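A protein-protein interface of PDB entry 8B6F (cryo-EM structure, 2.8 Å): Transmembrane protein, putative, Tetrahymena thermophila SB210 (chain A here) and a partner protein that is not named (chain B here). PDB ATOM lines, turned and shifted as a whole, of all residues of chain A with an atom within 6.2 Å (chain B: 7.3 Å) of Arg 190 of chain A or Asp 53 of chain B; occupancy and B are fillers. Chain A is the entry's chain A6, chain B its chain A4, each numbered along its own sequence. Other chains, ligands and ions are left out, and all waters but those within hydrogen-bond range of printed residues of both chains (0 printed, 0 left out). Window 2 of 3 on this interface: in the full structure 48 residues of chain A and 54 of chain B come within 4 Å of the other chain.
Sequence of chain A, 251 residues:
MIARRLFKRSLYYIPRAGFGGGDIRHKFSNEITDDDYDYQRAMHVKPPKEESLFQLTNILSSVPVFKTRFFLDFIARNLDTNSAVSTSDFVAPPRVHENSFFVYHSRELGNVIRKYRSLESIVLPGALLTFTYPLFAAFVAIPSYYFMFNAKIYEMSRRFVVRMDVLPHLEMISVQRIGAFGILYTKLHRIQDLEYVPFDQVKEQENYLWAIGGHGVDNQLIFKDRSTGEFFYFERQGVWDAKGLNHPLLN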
ATOM      1  N   LEU A 170     -10.610  14.575 -28.997  1.00  0.00           N
ATOM      2  CA  LEU A 170     -11.335  13.436 -28.451  1.00  0.00           C
ATOM      3  C   LEU A 170     -10.939  12.112 -29.089  1.00  0.00           C
ATOM      4  O   LEU A 170     -11.268  11.057 -28.536  1.00  0.00           O
ATOM      5  CB  LEU A 170     -12.839  13.636 -28.639  1.00  0.00           C
ATOM      6  CG  LEU A 170     -13.510  14.700 -27.777  1.00  0.00           C
ATOM      7  CD1 LEU A 170     -14.923  14.961 -28.262  1.00  0.00           C
ATOM      8  CD2 LEU A 170     -13.507  14.269 -26.322  1.00  0.00           C
ATOM      9  N   GLU A 171     -10.242  12.138 -30.223  1.00  0.00           N
ATOM     10  CA  GLU A 171      -9.999  10.935 -31.013  1.00  0.00           C
ATOM     11  C   GLU A 171     -11.311  10.222 -31.325  1.00  0.00           C
ATOM     12  O   GLU A 171     -11.422   9.000 -31.218  1.00  0.00           O
ATOM     13  CB  GLU A 171      -9.025   9.996 -30.299  1.00  0.00           C
ATOM     14  CG  GLU A 171      -7.612  10.547 -30.194  1.00  0.00           C
ATOM     15  CD  GLU A 171      -6.646   9.556 -29.576  1.00  0.00           C
ATOM     16  OE1 GLU A 171      -7.066   8.418 -29.284  1.00  0.00           O
ATOM     17  OE2 GLU A 171      -5.467   9.918 -29.383  1.00  0.00           O
ATOM     18  N   MET A 172     -12.320  11.001 -31.709  1.00  0.00           N
ATOM     19  CA  MET A 172     -13.657  10.505 -31.993  1.00  0.00           C
ATOM     20  C   MET A 172     -14.057  10.885 -33.411  1.00  0.00           C
ATOM     21  O   MET A 172     -13.398  11.684 -34.079  1.00  0.00           O
ATOM     22  CB  MET A 172     -14.680  11.064 -30.996  1.00  0.00           C
ATOM     23  CG  MET A 172     -14.720  10.337 -29.668  1.00  0.00           C
ATOM     24  SD  MET A 172     -16.063  10.926 -28.623  1.00  0.00           S
ATOM     25  CE  MET A 172     -15.950   9.786 -27.251  1.00  0.00           C
ATOM     26  N   ILE A 173     -15.163  10.301 -33.864  1.00  0.00           N
ATOM     27  CA  ILE A 173     -15.753  10.601 -35.163  1.00  0.00           C
ATOM     28  C   ILE A 173     -17.192  11.038 -34.934  1.00  0.00           C
ATOM     29  O   ILE A 173     -17.962  10.334 -34.271  1.00  0.00           O
ATOM     30  CB  ILE A 173     -15.684   9.399 -36.123  1.00  0.00           C
ATOM     31  CG1 ILE A 173     -14.256   8.845 -36.142  1.00  0.00           C
ATOM     32  CG2 ILE A 173     -16.145   9.803 -37.512  1.00  0.00           C
ATOM     33  CD1 ILE A 173     -13.962   7.876 -37.270  1.00  0.00           C
ATOM     34  N   LEU A 188     -21.398  10.989 -31.562  1.00  0.00           N
ATOM     35  CA  LEU A 188     -19.968  10.735 -31.469  1.00  0.00           C
ATOM     36  C   LEU A 188     -19.699   9.253 -31.248  1.00  0.00           C
ATOM     37  O   LEU A 188     -20.406   8.592 -30.481  1.00  0.00           O
ATOM     38  CB  LEU A 188     -19.341  11.538 -30.329  1.00  0.00           C
ATOM     39  CG  LEU A 188     -19.341  13.061 -30.459  1.00  0.00           C
ATOM     40  CD1 LEU A 188     -18.729  13.672 -29.219  1.00  0.00           C
ATOM     41  CD2 LEU A 188     -18.593  13.517 -31.701  1.00  0.00           C
ATOM     42  N   HIS A 189     -18.671   8.737 -31.919  1.00  0.00           N
ATOM     43  CA  HIS A 189     -18.248   7.353 -31.748  1.00  0.00           C
ATOM     44  C   HIS A 189     -16.730   7.304 -31.667  1.00  0.00           C
ATOM     45  O   HIS A 189     -16.045   7.950 -32.464  1.00  0.00           O
ATOM     46  CB  HIS A 189     -18.744   6.472 -32.899  1.00  0.00           C
ATOM     47  CG  HIS A 189     -20.230   6.484 -33.068  1.00  0.00           C
ATOM     48  ND1 HIS A 189     -20.884   7.431 -33.827  1.00  0.00           N
ATOM     49  CD2 HIS A 189     -21.191   5.671 -32.571  1.00  0.00           C
ATOM     50  CE1 HIS A 189     -22.183   7.196 -33.793  1.00  0.00           C
ATOM     51  NE2 HIS A 189     -22.397   6.135 -33.038  1.00  0.00           N
ATOM     52  N   ARG A 190     -16.211   6.541 -30.710  1.00  0.00           N
ATOM     53  CA  ARG A 190     -14.769   6.431 -30.544  1.00  0.00           C
ATOM     54  C   ARG A 190     -14.149   5.672 -31.709  1.00  0.00           C
ATOM     55  O   ARG A 190     -14.705   4.686 -32.197  1.00  0.00           O
ATOM     56  CB  ARG A 190     -14.432   5.727 -29.231  1.00  0.00           C
ATOM     57  CG  ARG A 190     -14.863   6.488 -27.992  1.00  0.00           C
ATOM     58  CD  ARG A 190     -14.320   5.842 -26.730  1.00  0.00           C
ATOM     59  NE  ARG A 190     -12.863   5.890 -26.683  1.00  0.00           N
ATOM     60  CZ  ARG A 190     -12.123   5.327 -25.739  1.00  0.00           C
ATOM     61  NH1 ARG A 190     -12.669   4.653 -24.742  1.00  0.00           N
ATOM     62  NH2 ARG A 190     -10.800   5.444 -25.799  1.00  0.00           N
ATOM     63  N   ILE A 191     -12.978   6.135 -32.152  1.00  0.00           N
ATOM     64  CA  ILE A 191     -12.273   5.451 -33.231  1.00  0.00           C
ATOM     65  C   ILE A 191     -11.844   4.059 -32.792  1.00  0.00           C
ATOM     66  O   ILE A 191     -11.697   3.155 -33.622  1.00  0.00           O
ATOM     67  CB  ILE A 191     -11.071   6.295 -33.700  1.00  0.00           C
ATOM     68  CG1 ILE A 191     -11.558   7.624 -34.281  1.00  0.00           C
ATOM     69  CG2 ILE A 191     -10.251   5.533 -34.738  1.00  0.00           C
ATOM     70  CD1 ILE A 191     -10.453   8.626 -34.541  1.00  0.00           C
ATOM     71  N   GLN A 192     -11.628   3.862 -31.490  1.00  0.00           N
ATOM     72  CA  GLN A 192     -11.227   2.551 -30.993  1.00  0.00           C
ATOM     73  C   GLN A 192     -12.374   1.551 -31.008  1.00  0.00           C
ATOM     74  O   GLN A 192     -12.129   0.347 -30.896  1.00  0.00           O
ATOM     75  CB  GLN A 192     -10.665   2.669 -29.575  1.00  0.00           C
ATOM     76  CG  GLN A 192      -9.345   3.420 -29.482  1.00  0.00           C
ATOM     77  CD  GLN A 192      -9.499   4.912 -29.692  1.00  0.00           C
ATOM     78  OE1 GLN A 192     -10.611   5.437 -29.713  1.00  0.00           O
ATOM     79  NE2 GLN A 192      -8.376   5.606 -29.851  1.00  0.00           N
ATOM     80  N   ASP A 193     -13.615   2.018 -31.139  1.00  0.00           N
ATOM     81  CA  ASP A 193     -14.781   1.147 -31.137  1.00  0.00           C
ATOM     82  C   ASP A 193     -15.318   0.868 -32.532  1.00  0.00           C
ATOM     83  O   ASP A 193     -16.362   0.220 -32.659  1.00  0.00           O
ATOM     84  CB  ASP A 193     -15.889   1.758 -30.274  1.00  0.00           C
ATOM     85  CG  ASP A 193     -15.491   1.880 -28.816  1.00  0.00           C
ATOM     86  OD1 ASP A 193     -14.355   1.487 -28.476  1.00  0.00           O
ATOM     87  OD2 ASP A 193     -16.310   2.368 -28.011  1.00  0.00           O
ATOM     88  N   LEU A 194     -14.642   1.337 -33.576  1.00  0.00           N
ATOM     89  CA  LEU A 194     -15.073   1.099 -34.945  1.00  0.00           C
ATOM     90  C   LEU A 194     -14.465  -0.189 -35.478  1.00  0.00           C
ATOM     91  O   LEU A 194     -13.280  -0.462 -35.275  1.00  0.00           O
ATOM     92  CB  LEU A 194     -14.680   2.266 -35.847  1.00  0.00           C
ATOM     93  CG  LEU A 194     -15.328   3.605 -35.507  1.00  0.00           C
ATOM     94  CD1 LEU A 194     -14.815   4.668 -36.435  1.00  0.00           C
ATOM     95  CD2 LEU A 194     -16.845   3.536 -35.581  1.00  0.00           C
ATOM     96  N   ASP A 225     -20.076   0.273 -34.901  1.00  0.00           N
ATOM     97  CA  ASP A 225     -19.533   0.572 -33.584  1.00  0.00           C
ATOM     98  C   ASP A 225     -19.781  -0.623 -32.670  1.00  0.00           C
ATOM     99  O   ASP A 225     -20.934  -0.968 -32.391  1.00  0.00           O
ATOM    100  CB  ASP A 225     -20.177   1.835 -33.014  1.00  0.00           C
ATOM    101  CG  ASP A 225     -19.577   2.247 -31.688  1.00  0.00           C
ATOM    102  OD1 ASP A 225     -18.438   2.756 -31.683  1.00  0.00           O
ATOM    103  OD2 ASP A 225     -20.245   2.062 -30.649  1.00  0.00           O
ATOM    104  N   PRO B  35     -18.529  14.587 -25.299  1.00  0.00           N
ATOM    105  CA  PRO B  35     -18.970  13.282 -24.793  1.00  0.00           C
ATOM    106  C   PRO B  35     -19.324  13.247 -23.314  1.00  0.00           C
ATOM    107  O   PRO B  35     -19.456  12.152 -22.763  1.00  0.00           O
ATOM    108  CB  PRO B  35     -17.751  12.393 -25.075  1.00  0.00           C
ATOM    109  CG  PRO B  35     -16.609  13.300 -24.912  1.00  0.00           C
ATOM    110  CD  PRO B  35     -17.061  14.654 -25.405  1.00  0.00           C
ATOM    111  N   PHE B  38     -21.678  10.587 -21.411  1.00  0.00           N
ATOM    112  CA  PHE B  38     -21.702   9.327 -22.145  1.00  0.00           C
ATOM    113  C   PHE B  38     -21.314   8.161 -21.248  1.00  0.00           C
ATOM    114  O   PHE B  38     -21.938   7.095 -21.302  1.00  0.00           O
ATOM    115  CB  PHE B  38     -20.763   9.390 -23.352  1.00  0.00           C
ATOM    116  CG  PHE B  38     -21.282  10.211 -24.499  1.00  0.00           C
ATOM    117  CD1 PHE B  38     -22.461  10.932 -24.393  1.00  0.00           C
ATOM    118  CD2 PHE B  38     -20.590  10.244 -25.698  1.00  0.00           C
ATOM    119  CE1 PHE B  38     -22.931  11.678 -25.455  1.00  0.00           C
ATOM    120  CE2 PHE B  38     -21.053  10.988 -26.765  1.00  0.00           C
ATOM    121  CZ  PHE B  38     -22.225  11.706 -26.645  1.00  0.00           C
ATOM    122  N   TYR B  39     -20.289   8.341 -20.419  1.00  0.00           N
ATOM    123  CA  TYR B  39     -19.715   7.254 -19.637  1.00  0.00           C
ATOM    124  C   TYR B  39     -19.904   7.473 -18.140  1.00  0.00           C
ATOM    125  O   TYR B  39     -19.134   6.958 -17.330  1.00  0.00           O
ATOM    126  CB  TYR B  39     -18.234   7.091 -19.969  1.00  0.00           C
ATOM    127  CG  TYR B  39     -17.954   7.091 -21.453  1.00  0.00           C
ATOM    128  CD1 TYR B  39     -18.218   5.971 -22.229  1.00  0.00           C
ATOM    129  CD2 TYR B  39     -17.420   8.210 -22.077  1.00  0.00           C
ATOM    130  CE1 TYR B  39     -17.965   5.966 -23.586  1.00  0.00           C
ATOM    131  CE2 TYR B  39     -17.161   8.216 -23.434  1.00  0.00           C
ATOM    132  CZ  TYR B  39     -17.436   7.090 -24.181  1.00  0.00           C
ATOM    133  OH  TYR B  39     -17.180   7.089 -25.532  1.00  0.00           O
ATOM    134  N   LEU B  48     -15.144   0.149 -11.970  1.00  0.00           N
ATOM    135  CA  LEU B  48     -15.217   0.989 -13.162  1.00  0.00           C
ATOM    136  C   LEU B  48     -13.978   0.836 -14.029  1.00  0.00           C
ATOM    137  O   LEU B  48     -14.050   1.008 -15.250  1.00  0.00           O
ATOM    138  CB  LEU B  48     -15.398   2.459 -12.777  1.00  0.00           C
ATOM    139  CG  LEU B  48     -16.788   2.927 -12.337  1.00  0.00           C
ATOM    140  CD1 LEU B  48     -17.814   2.752 -13.450  1.00  0.00           C
ATOM    141  CD2 LEU B  48     -17.222   2.200 -11.087  1.00  0.00           C
ATOM    142  N   ALA B  49     -12.836   0.517 -13.420  1.00  0.00           N
ATOM    143  CA  ALA B  49     -11.613   0.352 -14.196  1.00  0.00           C
ATOM    144  C   ALA B  49     -11.738  -0.808 -15.175  1.00  0.00           C
ATOM    145  O   ALA B  49     -11.229  -0.738 -16.299  1.00  0.00           O
ATOM    146  CB  ALA B  49     -10.429   0.136 -13.254  1.00  0.00           C
ATOM    147  N   ASN B  50     -12.408  -1.885 -14.764  1.00  0.00           N
ATOM    148  CA  ASN B  50     -12.534  -3.050 -15.635  1.00  0.00           C
ATOM    149  C   ASN B  50     -13.305  -2.714 -16.905  1.00  0.00           C
ATOM    150  O   ASN B  50     -12.940  -3.163 -17.998  1.00  0.00           O
ATOM    151  CB  ASN B  50     -13.223  -4.191 -14.888  1.00  0.00           C
ATOM    152  CG  ASN B  50     -12.417  -4.685 -13.706  1.00  0.00           C
ATOM    153  OD1 ASN B  50     -11.188  -4.626 -13.708  1.00  0.00           O
ATOM    154  ND2 ASN B  50     -13.108  -5.182 -12.688  1.00  0.00           N
ATOM    155  N   GLU B  51     -14.373  -1.928 -16.783  1.00  0.00           N
ATOM    156  CA  GLU B  51     -15.272  -1.694 -17.906  1.00  0.00           C
ATOM    157  C   GLU B  51     -14.909  -0.458 -18.717  1.00  0.00           C
ATOM    158  O   GLU B  51     -15.097  -0.457 -19.939  1.00  0.00           O
ATOM    159  CB  GLU B  51     -16.712  -1.566 -17.398  1.00  0.00           C
ATOM    160  CG  GLU B  51     -17.781  -1.852 -18.449  1.00  0.00           C
ATOM    161  CD  GLU B  51     -17.964  -0.719 -19.441  1.00  0.00           C
ATOM    162  OE1 GLU B  51     -17.611   0.431 -19.110  1.00  0.00           O
ATOM    163  OE2 GLU B  51     -18.466  -0.980 -20.555  1.00  0.00           O
ATOM    164  N   MET B  52     -14.388   0.587 -18.079  1.00  0.00           N
ATOM    165  CA  MET B  52     -14.155   1.863 -18.736  1.00  0.00           C
ATOM    166  C   MET B  52     -12.664   2.152 -18.856  1.00  0.00           C
ATOM    167  O   MET B  52     -11.828   1.535 -18.189  1.00  0.00           O
ATOM    168  CB  MET B  52     -14.847   2.999 -17.974  1.00  0.00           C
ATOM    169  CG  MET B  52     -16.363   2.882 -17.960  1.00  0.00           C
ATOM    170  SD  MET B  52     -17.175   4.290 -17.187  1.00  0.00           S
ATOM    171  CE  MET B  52     -18.894   3.825 -17.375  1.00  0.00           C
ATOM    172  N   ASP B  53     -12.346   3.104 -19.727  1.00  0.00           N
ATOM    173  CA  ASP B  53     -10.980   3.518 -20.002  1.00  0.00           C
ATOM    174  C   ASP B  53     -10.662   4.815 -19.261  1.00  0.00           C
ATOM    175  O   ASP B  53     -11.549   5.501 -18.748  1.00  0.00           O
ATOM    176  CB  ASP B  53     -10.788   3.691 -21.514  1.00  0.00           C
ATOM    177  CG  ASP B  53      -9.347   3.955 -21.898  1.00  0.00           C
ATOM    178  OD1 ASP B  53      -8.494   3.072 -21.668  1.00  0.00           O
ATOM    179  OD2 ASP B  53      -9.068   5.048 -22.435  1.00  0.00           O
ATOM    180  N   VAL B  54      -9.372   5.151 -19.215  1.00  0.00           N
ATOM    181  CA  VAL B  54      -8.953   6.378 -18.541  1.00  0.00           C
ATOM    182  C   VAL B  54      -9.615   7.589 -19.187  1.00  0.00           C
ATOM    183  O   VAL B  54      -9.983   8.552 -18.504  1.00  0.00           O
ATOM    184  CB  VAL B  54      -7.417   6.502 -18.551  1.00  0.00           C
ATOM    185  CG1 VAL B  54      -6.789   5.347 -17.790  1.00  0.00           C
ATOM    186  CG2 VAL B  54      -6.886   6.559 -19.976  1.00  0.00           C
ATOM    187  N   PHE B  55      -9.779   7.558 -20.510  1.00  0.00           N
ATOM    188  CA  PHE B  55     -10.439   8.661 -21.202  1.00  0.00           C
ATOM    189  C   PHE B  55     -11.865   8.834 -20.701  1.00  0.00           C
ATOM    190  O   PHE B  55     -12.285   9.944 -20.356  1.00  0.00           O
ATOM    191  CB  PHE B  55     -10.411   8.410 -22.712  1.00  0.00           C
ATOM    192  CG  PHE B  55     -11.396   9.237 -23.489  1.00  0.00           C
ATOM    193  CD1 PHE B  55     -11.093  10.540 -23.848  1.00  0.00           C
ATOM    194  CD2 PHE B  55     -12.613   8.707 -23.878  1.00  0.00           C
ATOM    195  CE1 PHE B  55     -11.990  11.301 -24.570  1.00  0.00           C
ATOM    196  CE2 PHE B  55     -13.515   9.463 -24.602  1.00  0.00           C
ATOM    197  CZ  PHE B  55     -13.204  10.763 -24.947  1.00  0.00           C
ATOM    198  N   GLN B  56     -12.621   7.737 -20.633  1.00  0.00           N
ATOM    199  CA  GLN B  56     -13.999   7.816 -20.159  1.00  0.00           C
ATOM    200  C   GLN B  56     -14.060   8.288 -18.712  1.00  0.00           C
ATOM    201  O   GLN B  56     -14.885   9.138 -18.361  1.00  0.00           O
ATOM    202  CB  GLN B  56     -14.675   6.454 -20.305  1.00  0.00           C
ATOM    203  CG  GLN B  56     -14.632   5.894 -21.716  1.00  0.00           C
ATOM    204  CD  GLN B  56     -15.159   4.476 -21.791  1.00  0.00           C
ATOM    205  OE1 GLN B  56     -15.424   3.846 -20.771  1.00  0.00           O
ATOM    206  NE2 GLN B  56     -15.320   3.971 -23.008  1.00  0.00           N
ATOM    207  N   LEU B  57     -13.197   7.740 -17.857  1.00  0.00           N
ATOM    208  CA  LEU B  57     -13.197   8.132 -16.452  1.00  0.00           C
ATOM    209  C   LEU B  57     -12.841   9.604 -16.293  1.00  0.00           C
ATOM    210  O   LEU B  57     -13.419  10.305 -15.454  1.00  0.00           O
ATOM    211  CB  LEU B  57     -12.234   7.252 -15.657  1.00  0.00           C
ATOM    212  CG  LEU B  57     -12.567   5.758 -15.616  1.00  0.00           C
ATOM    213  CD1 LEU B  57     -11.511   5.008 -14.832  1.00  0.00           C
ATOM    214  CD2 LEU B  57     -13.943   5.506 -15.022  1.00  0.00           C
ATOM    215  N   GLY B  58     -11.890  10.093 -17.090  1.00  0.00           N
ATOM    216  CA  GLY B  58     -11.536  11.501 -17.021  1.00  0.00           C
ATOM    217  C   GLY B  58     -12.666  12.409 -17.465  1.00  0.00           C
ATOM    218  O   GLY B  58     -12.906  13.454 -16.853  1.00  0.00           O
ATOM    219  N   LEU B  59     -13.373  12.033 -18.531  1.00  0.00           N
ATOM    220  CA  LEU B  59     -14.534  12.816 -18.943  1.00  0.00           C
ATOM    221  C   LEU B  59     -15.559  12.885 -17.821  1.00  0.00           C
ATOM    222  O   LEU B  59     -16.071  13.961 -17.494  1.00  0.00           O
ATOM    223  CB  LEU B  59     -15.158  12.214 -20.205  1.00  0.00           C
ATOM    224  CG  LEU B  59     -14.697  12.768 -21.558  1.00  0.00           C
ATOM    225  CD1 LEU B  59     -15.077  14.232 -21.706  1.00  0.00           C
ATOM    226  CD2 LEU B  59     -13.203  12.591 -21.751  1.00  0.00           C
ATOM    227  N   ILE B 105      -9.132   6.125 -11.715  1.00  0.00           N
ATOM    228  CA  ILE B 105      -8.159   6.690 -12.647  1.00  0.00           C
ATOM    229  C   ILE B 105      -6.747   6.521 -12.104  1.00  0.00           C
ATOM    230  O   ILE B 105      -5.827   6.134 -12.834  1.00  0.00           O
ATOM    231  CB  ILE B 105      -8.482   8.170 -12.924  1.00  0.00           C
ATOM    232  CG1 ILE B 105      -9.782   8.287 -13.717  1.00  0.00           C
ATOM    233  CG2 ILE B 105      -7.340   8.835 -13.684  1.00  0.00           C
ATOM    234  CD1 ILE B 105     -10.298   9.703 -13.832  1.00  0.00           C
ATOM    235  N   LEU B 108      -5.652   2.944 -12.443  1.00  0.00           N
ATOM    236  CA  LEU B 108      -5.275   2.626 -13.817  1.00  0.00           C
ATOM    237  C   LEU B 108      -3.896   3.177 -14.151  1.00  0.00           C
ATOM    238  O   LEU B 108      -3.072   2.480 -14.754  1.00  0.00           O
ATOM    239  CB  LEU B 108      -6.317   3.176 -14.792  1.00  0.00           C
ATOM    240  CG  LEU B 108      -7.659   2.442 -14.863  1.00  0.00           C
ATOM    241  CD1 LEU B 108      -8.611   3.169 -15.791  1.00  0.00           C
ATOM    242  CD2 LEU B 108      -7.469   1.005 -15.327  1.00  0.00           C
ATOM    243  N   LYS B 113      -1.808   1.647 -17.685  1.00  0.00           N
ATOM    244  CA  LYS B 113      -2.606   2.034 -18.847  1.00  0.00           C
ATOM    245  C   LYS B 113      -2.699   3.554 -18.861  1.00  0.00           C
ATOM    246  O   LYS B 113      -3.460   4.149 -18.096  1.00  0.00           O
ATOM    247  CB  LYS B 113      -3.985   1.386 -18.795  1.00  0.00           C
ATOM    248  CG  LYS B 113      -3.946  -0.135 -18.806  1.00  0.00           C
ATOM    249  CD  LYS B 113      -5.345  -0.728 -18.848  1.00  0.00           C
ATOM    250  CE  LYS B 113      -5.303  -2.248 -18.854  1.00  0.00           C
ATOM    251  NZ  LYS B 113      -4.565  -2.789 -20.029  1.00  0.00           N
ATOM    252  N   LYS B 114      -1.920   4.188 -19.742  1.00  0.00           N
ATOM    253  CA  LYS B 114      -1.791   5.638 -19.764  1.00  0.00           C
ATOM    254  C   LYS B 114      -2.152   6.283 -21.093  1.00  0.00           C
ATOM    255  O   LYS B 114      -2.423   7.488 -21.113  1.00  0.00           O
ATOM    256  CB  LYS B 114      -0.354   6.051 -19.404  1.00  0.00           C
ATOM    257  CG  LYS B 114       0.141   5.486 -18.080  1.00  0.00           C
ATOM    258  CD  LYS B 114       1.577   5.906 -17.803  1.00  0.00           C
ATOM    259  CE  LYS B 114       2.074   5.332 -16.485  1.00  0.00           C
ATOM    260  NZ  LYS B 114       3.468   5.763 -16.179  1.00  0.00           N
ATOM    261  N   GLU B 115      -2.166   5.533 -22.193  1.00  0.00           N
ATOM    262  CA  GLU B 115      -2.461   6.125 -23.491  1.00  0.00           C
ATOM    263  C   GLU B 115      -3.886   6.661 -23.511  1.00  0.00           C
ATOM    264  O   GLU B 115      -4.838   5.944 -23.190  1.00  0.00           O
ATOM    265  CB  GLU B 115      -2.264   5.093 -24.600  1.00  0.00           C
ATOM    266  CG  GLU B 115      -2.566   5.624 -25.991  1.00  0.00           C
ATOM    267  CD  GLU B 115      -2.196   4.639 -27.082  1.00  0.00           C
ATOM    268  OE1 GLU B 115      -1.559   3.612 -26.765  1.00  0.00           O
ATOM    269  OE2 GLU B 115      -2.540   4.893 -28.255  1.00  0.00           O
ATOM    270  N   CYS B 116      -4.031   7.925 -23.898  1.00  0.00           N
ATOM    271  CA  CYS B 116      -5.324   8.590 -23.874  1.00  0.00           C
ATOM    272  C   CYS B 116      -5.260   9.811 -24.783  1.00  0.00           C
ATOM    273  O   CYS B 116      -4.167  10.286 -25.111  1.00  0.00           O
ATOM    274  CB  CYS B 116      -5.701   8.999 -22.443  1.00  0.00           C
ATOM    275  SG  CYS B 116      -4.501  10.111 -21.672  1.00  0.00           S
ATOM    276  N   PRO B 117      -6.416  10.339 -25.211  1.00  0.00           N
ATOM    277  CA  PRO B 117      -6.411  11.566 -26.022  1.00  0.00           C
ATOM    278  C   PRO B 117      -5.985  12.800 -25.241  1.00  0.00           C
ATOM    279  O   PRO B 117      -5.697  12.725 -24.044  1.00  0.00           O
ATOM    280  CB  PRO B 117      -7.867  11.685 -26.494  1.00  0.00           C
ATOM    281  CG  PRO B 117      -8.447  10.328 -26.329  1.00  0.00           C
ATOM    282  CD  PRO B 117      -7.756   9.732 -25.150  1.00  0.00           C
ATOM    283  N   THR B 120      -8.268  13.887 -22.342  1.00  0.00           N
ATOM    284  CA  THR B 120      -8.042  13.165 -21.096  1.00  0.00           C
ATOM    285  C   THR B 120      -7.022  13.901 -20.237  1.00  0.00           C
ATOM    286  O   THR B 120      -7.219  14.075 -19.030  1.00  0.00           O
ATOM    287  CB  THR B 120      -7.586  11.736 -21.385  1.00  0.00           C
ATOM    288  OG1 THR B 120      -8.576  11.076 -22.180  1.00  0.00           O
ATOM    289  CG2 THR B 120      -7.391  10.961 -20.088  1.00  0.00           C
ATOM    290  N   ARG B 269     -26.342   6.365 -24.302  1.00  0.00           N
ATOM    291  CA  ARG B 269     -25.219   6.749 -23.454  1.00  0.00           C
ATOM    292  C   ARG B 269     -25.582   7.914 -22.538  1.00  0.00           C
ATOM    293  O   ARG B 269     -25.201   7.928 -21.362  1.00  0.00           O
ATOM    294  CB  ARG B 269     -24.011   7.098 -24.321  1.00  0.00           C
ATOM    295  CG  ARG B 269     -23.430   5.901 -25.059  1.00  0.00           C
ATOM    296  CD  ARG B 269     -22.454   6.324 -26.141  1.00  0.00           C
ATOM    297  NE  ARG B 269     -23.122   7.019 -27.235  1.00  0.00           N
ATOM    298  CZ  ARG B 269     -22.528   7.398 -28.357  1.00  0.00           C
ATOM    299  NH1 ARG B 269     -21.244   7.164 -28.573  1.00  0.00           N
ATOM    300  NH2 ARG B 269     -23.240   8.023 -29.290  1.00  0.00           N
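OD2 of Asp 53 of chain B is in salt-bridge range of NH2 of Arg 190 of chain A (3.8 Å).
The side-chain amide nitrogen (NE2) of Gln 56 of chain B sits close to the guanidinium group (NH1) of Arg 190 of chain A (3.2 Å).
The guanidinium group of Arg 269 of chain B is in hydrogen-bond range of the backbone carbonyl oxygen of Leu 188 of chain A (2.5 Å).
The side-chain carboxylate (OD2) of Asp 53 of chain B sits close to the backbone NH (N) of Phe 55 of chain B, 3.2 Å away.
N of Asp 53 of chain B lies within hydrogen-bond range of OE1 of Gln 56 of chain B, 3.3 Å away.
The backbone carbonyl oxygen (O) of Glu 171 of chain A lies close to the backbone NH (N) of Ile 191 of chain A (3.4 Å).
OE1 of Glu 171 of chain A is in hydrogen-bond range of NE2 of Gln 192 of chain A (3.2 Å).
CG of Pro 35 of chain B touches CD2 of Leu 170 of chain A, 3.5 Å away.
Leu 170 of chain A touches Phe 55 of chain B (CD2 to CE1, 3.8 Å).
Pro 117 of chain B touches Leu 170 of chain A.
Glu 171 of chain A touches Pro 117 of chain B (OE1 to CG, 3.8 Å).
Pro 35 of chain B touches Met 172 of chain A (CB to CE, 3.8 Å).
Tyr 39 of chain B touches Met 172 of chain A (OH to CE, 3.4 Å).
Met 172 of chain A touches Phe 55 of chain B.
Leu 188 of chain A touches Phe 38 of chain B.
CD of Arg 190 of chain A touches OH of Tyr 39 of chain B, 3.3 Å away.
Arg 190 of chain A touches Phe 55 of chain B (CZ to CD2, 3.9 Å).
Arg 190 of chain A touches just these residues of chain B: Tyr 39 (3.3 Å), Asp 53 (3.8 Å), Phe 55 (3.9 Å) and Gln 56 (3.2 Å).
Of the printed residues of chain A, Pro 35 of chain B touches Leu 170 and Met 172.
Of the printed residues of chain B, Met 172 of chain A touches Pro 35, Tyr 39 and Phe 55.
Of the printed residues of chain A, Gln 56 of chain B touches Arg 190 (3.2 Å).
Of the printed residues of chain A, Pro 117 of chain B touches Leu 170 (3.7 Å) and Glu 171 (3.8 Å).
Ile 105 of chain B touches none of the printed residues of chain A.
Asp 225 of chain A touches none of the printed residues of chain B.
The nearest printed residue of chain A that does not touch Asp 53 of chain B is Gln 192 of chain A (7.2 Å).
Of the 12 printed residues of chain A, 5 touch a printed residue of chain B.
Hydrophobic or aromatic side chains of chain A within 4 Å of the printed part of chain B: Leu 170, Met 172 and Leu 188.
Of the 24 printed residues of chain B, 8 touch a printed residue of chain A.
Hydrophobic or aromatic side chains of chain B that line the printed part of chain A: Pro 35, Phe 38, Tyr 39, Phe 55 and Pro 117.
Among the printed residues, Asp or Glu carboxylates within 4 Å of a Lys or Arg side-chain nitrogen of the other chain: Arg 190 of chain A with Asp 53 of chain B (3.8 Å).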
